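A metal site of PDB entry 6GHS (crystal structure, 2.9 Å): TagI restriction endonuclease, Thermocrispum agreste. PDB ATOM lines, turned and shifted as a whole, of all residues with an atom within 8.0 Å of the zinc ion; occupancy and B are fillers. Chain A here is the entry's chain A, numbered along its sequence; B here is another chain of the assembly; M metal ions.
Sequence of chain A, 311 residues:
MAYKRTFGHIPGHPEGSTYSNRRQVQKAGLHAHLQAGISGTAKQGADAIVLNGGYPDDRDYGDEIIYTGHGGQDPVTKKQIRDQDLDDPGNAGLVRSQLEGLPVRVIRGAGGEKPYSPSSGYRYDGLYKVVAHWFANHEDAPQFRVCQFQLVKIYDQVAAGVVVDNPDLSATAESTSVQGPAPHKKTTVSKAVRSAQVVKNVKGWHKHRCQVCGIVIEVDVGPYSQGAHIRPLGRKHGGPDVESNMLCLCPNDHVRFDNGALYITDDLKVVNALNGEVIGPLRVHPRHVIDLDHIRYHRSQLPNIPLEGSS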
ATOM      1  N   ARG A 209      26.249 -10.161 -33.543  1.00  0.00           N
ATOM      2  CA  ARG A 209      26.885 -11.409 -33.138  1.00  0.00           C
ATOM      3  C   ARG A 209      27.569 -11.160 -31.842  1.00  0.00           C
ATOM      4  O   ARG A 209      28.293 -10.175 -31.688  1.00  0.00           O
ATOM      5  CB  ARG A 209      27.941 -11.873 -34.133  1.00  0.00           C
ATOM      6  CG  ARG A 209      27.374 -12.506 -35.383  1.00  0.00           C
ATOM      7  CD  ARG A 209      28.464 -12.865 -36.387  1.00  0.00           C
ATOM      8  NE  ARG A 209      29.016 -14.196 -36.124  1.00  0.00           N
ATOM      9  CZ  ARG A 209      28.499 -15.360 -36.553  1.00  0.00           C
ATOM     10  NH1 ARG A 209      27.367 -15.405 -37.276  1.00  0.00           N
ATOM     11  NH2 ARG A 209      29.119 -16.498 -36.236  1.00  0.00           N
ATOM     12  N   CYS A 210      27.359 -12.080 -30.896  1.00  0.00           N
ATOM     13  CA  CYS A 210      28.033 -12.018 -29.629  1.00  0.00           C
ATOM     14  C   CYS A 210      29.520 -12.172 -29.849  1.00  0.00           C
ATOM     15  O   CYS A 210      29.974 -13.113 -30.513  1.00  0.00           O
ATOM     16  CB  CYS A 210      27.550 -13.122 -28.709  1.00  0.00           C
ATOM     17  SG  CYS A 210      28.270 -12.978 -27.069  1.00  0.00           S
ATOM     18  N   GLN A 211      30.275 -11.245 -29.257  1.00  0.00           N
ATOM     19  CA  GLN A 211      31.722 -11.283 -29.350  1.00  0.00           C
ATOM     20  C   GLN A 211      32.331 -12.469 -28.567  1.00  0.00           C
ATOM     21  O   GLN A 211      33.478 -12.838 -28.799  1.00  0.00           O
ATOM     22  CB  GLN A 211      32.325  -9.946 -28.929  1.00  0.00           C
ATOM     23  CG  GLN A 211      31.987  -8.796 -29.867  1.00  0.00           C
ATOM     24  CD  GLN A 211      32.744  -7.509 -29.580  1.00  0.00           C
ATOM     25  OE1 GLN A 211      32.137  -6.482 -29.280  1.00  0.00           O
ATOM     26  NE2 GLN A 211      34.077  -7.554 -29.681  1.00  0.00           N
ATOM     27  N   VAL A 212      31.567 -13.074 -27.668  1.00  0.00           N
ATOM     28  CA  VAL A 212      32.048 -14.204 -26.881  1.00  0.00           C
ATOM     29  C   VAL A 212      31.674 -15.564 -27.472  1.00  0.00           C
ATOM     30  O   VAL A 212      32.558 -16.380 -27.707  1.00  0.00           O
ATOM     31  CB  VAL A 212      31.546 -14.113 -25.430  1.00  0.00           C
ATOM     32  CG1 VAL A 212      32.001 -15.332 -24.644  1.00  0.00           C
ATOM     33  CG2 VAL A 212      32.014 -12.808 -24.791  1.00  0.00           C
ATOM     34  N   CYS A 213      30.365 -15.795 -27.695  1.00  0.00           N
ATOM     35  CA  CYS A 213      29.849 -17.123 -28.122  1.00  0.00           C
ATOM     36  C   CYS A 213      29.474 -17.213 -29.603  1.00  0.00           C
ATOM     37  O   CYS A 213      29.094 -18.292 -30.093  1.00  0.00           O
ATOM     38  CB  CYS A 213      28.662 -17.577 -27.243  1.00  0.00           C
ATOM     39  SG  CYS A 213      27.133 -16.655 -27.494  1.00  0.00           S
ATOM     40  N   GLY A 214      29.534 -16.098 -30.323  1.00  0.00           N
ATOM     41  CA  GLY A 214      29.319 -16.109 -31.758  1.00  0.00           C
ATOM     42  C   GLY A 214      27.891 -16.053 -32.256  1.00  0.00           C
ATOM     43  O   GLY A 214      27.682 -15.771 -33.441  1.00  0.00           O
ATOM     44  N   ILE A 215      26.884 -16.267 -31.398  1.00  0.00           N
ATOM     45  CA  ILE A 215      25.522 -16.355 -31.920  1.00  0.00           C
ATOM     46  C   ILE A 215      24.857 -15.031 -32.120  1.00  0.00           C
ATOM     47  O   ILE A 215      25.185 -14.043 -31.471  1.00  0.00           O
ATOM     48  CB  ILE A 215      24.565 -17.243 -31.100  1.00  0.00           C
ATOM     49  CG1 ILE A 215      24.266 -16.658 -29.716  1.00  0.00           C
ATOM     50  CG2 ILE A 215      25.111 -18.658 -30.988  1.00  0.00           C
ATOM     51  CD1 ILE A 215      23.004 -17.270 -29.133  1.00  0.00           C
ATOM     52  N   VAL A 216      23.887 -15.063 -33.030  1.00  0.00           N
ATOM     53  CA  VAL A 216      22.915 -14.026 -33.219  1.00  0.00           C
ATOM     54  C   VAL A 216      21.611 -14.561 -32.695  1.00  0.00           C
ATOM     55  O   VAL A 216      21.204 -15.662 -33.024  1.00  0.00           O
ATOM     56  CB  VAL A 216      22.724 -13.723 -34.716  1.00  0.00           C
ATOM     57  CG1 VAL A 216      21.864 -12.472 -34.884  1.00  0.00           C
ATOM     58  CG2 VAL A 216      24.058 -13.546 -35.423  1.00  0.00           C
ATOM     59  N   ILE A 217      20.941 -13.782 -31.870  1.00  0.00           N
ATOM     60  CA  ILE A 217      19.606 -14.093 -31.437  1.00  0.00           C
ATOM     61  C   ILE A 217      18.695 -13.570 -32.538  1.00  0.00           C
ATOM     62  O   ILE A 217      18.742 -12.393 -32.866  1.00  0.00           O
ATOM     63  CB  ILE A 217      19.307 -13.392 -30.099  1.00  0.00           C
ATOM     64  CG1 ILE A 217      20.277 -13.841 -29.003  1.00  0.00           C
ATOM     65  CG2 ILE A 217      17.874 -13.638 -29.649  1.00  0.00           C
ATOM     66  CD1 ILE A 217      20.126 -15.288 -28.588  1.00  0.00           C
ATOM     67  N   CYS A 248      29.433  -5.989 -28.213  1.00  0.00           N
ATOM     68  CA  CYS A 248      28.177  -6.623 -28.628  1.00  0.00           C
ATOM     69  C   CYS A 248      28.124  -8.049 -28.070  1.00  0.00           C
ATOM     70  O   CYS A 248      28.985  -8.872 -28.367  1.00  0.00           O
ATOM     71  CB  CYS A 248      28.087  -6.643 -30.153  1.00  0.00           C
ATOM     72  SG  CYS A 248      26.645  -7.469 -30.833  1.00  0.00           S
ATOM     73  N   LEU A 249      27.106  -8.339 -27.244  1.00  0.00           N
ATOM     74  CA  LEU A 249      26.950  -9.636 -26.594  1.00  0.00           C
ATOM     75  C   LEU A 249      25.515 -10.160 -26.633  1.00  0.00           C
ATOM     76  O   LEU A 249      24.572  -9.377 -26.656  1.00  0.00           O
ATOM     77  CB  LEU A 249      27.312  -9.536 -25.128  1.00  0.00           C
ATOM     78  CG  LEU A 249      28.687  -9.034 -24.747  1.00  0.00           C
ATOM     79  CD1 LEU A 249      28.763  -8.944 -23.240  1.00  0.00           C
ATOM     80  CD2 LEU A 249      29.757  -9.969 -25.278  1.00  0.00           C
ATOM     81  N   CYS A 250      25.352 -11.484 -26.558  1.00  0.00           N
ATOM     82  CA  CYS A 250      24.040 -12.086 -26.404  1.00  0.00           C
ATOM     83  C   CYS A 250      23.615 -11.833 -24.966  1.00  0.00           C
ATOM     84  O   CYS A 250      24.469 -11.572 -24.114  1.00  0.00           O
ATOM     85  CB  CYS A 250      24.061 -13.588 -26.681  1.00  0.00           C
ATOM     86  SG  CYS A 250      25.188 -14.490 -25.624  1.00  0.00           S
ATOM     87  N   PRO A 251      22.307 -11.906 -24.683  1.00  0.00           N
ATOM     88  CA  PRO A 251      21.837 -11.658 -23.314  1.00  0.00           C
ATOM     89  C   PRO A 251      22.473 -12.505 -22.218  1.00  0.00           C
ATOM     90  O   PRO A 251      22.725 -11.965 -21.156  1.00  0.00           O
ATOM     91  CB  PRO A 251      20.351 -11.960 -23.405  1.00  0.00           C
ATOM     92  CG  PRO A 251      20.010 -11.561 -24.790  1.00  0.00           C
ATOM     93  CD  PRO A 251      21.193 -11.887 -25.645  1.00  0.00           C
ATOM     94  N   ASN A 252      22.735 -13.792 -22.494  1.00  0.00           N
ATOM     95  CA  ASN A 252      23.389 -14.702 -21.532  1.00  0.00           C
ATOM     96  C   ASN A 252      24.801 -14.230 -21.191  1.00  0.00           C
ATOM     97  O   ASN A 252      25.151 -14.123 -20.018  1.00  0.00           O
ATOM     98  CB  ASN A 252      23.452 -16.172 -22.030  1.00  0.00           C
ATOM     99  CG  ASN A 252      22.090 -16.869 -22.010  1.00  0.00           C
ATOM    100  OD1 ASN A 252      21.067 -16.249 -21.770  1.00  0.00           O
ATOM    101  ND2 ASN A 252      22.079 -18.164 -22.289  1.00  0.00           N
ATOM    102  N   ASP A 253      25.601 -13.944 -22.209  1.00  0.00           N
ATOM    103  CA  ASP A 253      26.967 -13.490 -21.950  1.00  0.00           C
ATOM    104  C   ASP A 253      27.052 -12.108 -21.315  1.00  0.00           C
ATOM    105  O   ASP A 253      27.946 -11.868 -20.505  1.00  0.00           O
ATOM    106  CB  ASP A 253      27.844 -13.577 -23.215  1.00  0.00           C
ATOM    107  CG  ASP A 253      28.148 -15.019 -23.605  1.00  0.00           C
ATOM    108  OD1 ASP A 253      28.293 -15.878 -22.717  1.00  0.00           O
ATOM    109  OD2 ASP A 253      28.237 -15.316 -24.802  1.00  0.00           O
ATOM    110  N   HIS A 254      26.102 -11.215 -21.626  1.00  0.00           N
ATOM    111  CA  HIS A 254      26.022  -9.914 -20.915  1.00  0.00           C
ATOM    112  C   HIS A 254      25.983 -10.131 -19.379  1.00  0.00           C
ATOM    113  O   HIS A 254      26.763  -9.533 -18.647  1.00  0.00           O
ATOM    114  CB  HIS A 254      24.796  -9.103 -21.383  1.00  0.00           C
ATOM    115  CG  HIS A 254      24.828  -7.649 -20.985  1.00  0.00           C
ATOM    116  ND1 HIS A 254      23.965  -6.718 -21.506  1.00  0.00           N
ATOM    117  CD2 HIS A 254      25.636  -6.963 -20.124  1.00  0.00           C
ATOM    118  CE1 HIS A 254      24.222  -5.538 -20.991  1.00  0.00           C
ATOM    119  NE2 HIS A 254      25.229  -5.654 -20.146  1.00  0.00           N
ATOM    120  N   ARG A 256      26.786 -12.785 -17.512  1.00  0.00           N
ATOM    121  CA  ARG A 256      28.058 -13.347 -17.040  1.00  0.00           C
ATOM    122  C   ARG A 256      29.129 -12.266 -16.920  1.00  0.00           C
ATOM    123  O   ARG A 256      29.781 -12.117 -15.895  1.00  0.00           O
ATOM    124  CB  ARG A 256      28.565 -14.441 -17.991  1.00  0.00           C
ATOM    125  CG  ARG A 256      27.631 -15.626 -18.151  1.00  0.00           C
ATOM    126  CD  ARG A 256      28.361 -16.833 -18.664  1.00  0.00           C
ATOM    127  NE  ARG A 256      27.399 -17.851 -19.091  1.00  0.00           N
ATOM    128  CZ  ARG A 256      27.281 -18.373 -20.325  1.00  0.00           C
ATOM    129  NH1 ARG A 256      28.090 -18.014 -21.325  1.00  0.00           N
ATOM    130  NH2 ARG A 256      26.354 -19.305 -20.558  1.00  0.00           N
ATOM    131  N   LEU A 262      33.229 -13.790 -16.557  1.00  0.00           N
ATOM    132  CA  LEU A 262      34.078 -13.655 -17.726  1.00  0.00           C
ATOM    133  C   LEU A 262      35.060 -12.512 -17.469  1.00  0.00           C
ATOM    134  O   LEU A 262      34.711 -11.523 -16.816  1.00  0.00           O
ATOM    135  CB  LEU A 262      33.236 -13.301 -18.941  1.00  0.00           C
ATOM    136  CG  LEU A 262      32.214 -14.336 -19.391  1.00  0.00           C
ATOM    137  CD1 LEU A 262      31.203 -13.720 -20.360  1.00  0.00           C
ATOM    138  CD2 LEU A 262      32.905 -15.560 -19.979  1.00  0.00           C
ATOM    139  N   ASN B 252      18.612 -15.514 -22.973  1.00  0.00           N
ATOM    140  CA  ASN B 252      18.453 -15.648 -24.435  1.00  0.00           C
ATOM    141  C   ASN B 252      17.062 -16.166 -24.799  1.00  0.00           C
ATOM    142  O   ASN B 252      16.384 -15.581 -25.640  1.00  0.00           O
ATOM    143  CB  ASN B 252      19.522 -16.571 -25.083  1.00  0.00           C
ATOM    144  CG  ASN B 252      20.912 -15.932 -25.131  1.00  0.00           C
ATOM    145  OD1 ASN B 252      21.141 -14.875 -24.568  1.00  0.00           O
ATOM    146  ND2 ASN B 252      21.850 -16.596 -25.791  1.00  0.00           N
HETATM  147 ZN    ZN M   1      27.233 -15.057 -26.369  1.00  0.00          ZN
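O of Ile 215 sits at hydrogen-bond distance from N of Cys 210 (3.0 Å). N of Val 212 lies close to SG of Cys 210 (3.4 Å). The side-chain carboxylate (OD1) of Asp 253 is in salt-bridge range of the guanidinium group (NH1) of Arg 256 (2.6 Å).
OD2 of Asp 253 is bound to the zinc ion, 1.9 Å away. The side-chain sulfur (SG) of Cys 213 is bound to the zinc ion, 2.0 Å away. The zinc ion is bound by SG of Cys 250 (2.2 Å). SG of Cys 210 is bound to the zinc ion (2.4 Å).
Of the 19 residues printed, 4 come within 4 Å of the zinc ion. The nearest printed residue that does not touch the zinc ion is Val 212 (4.5 Å).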
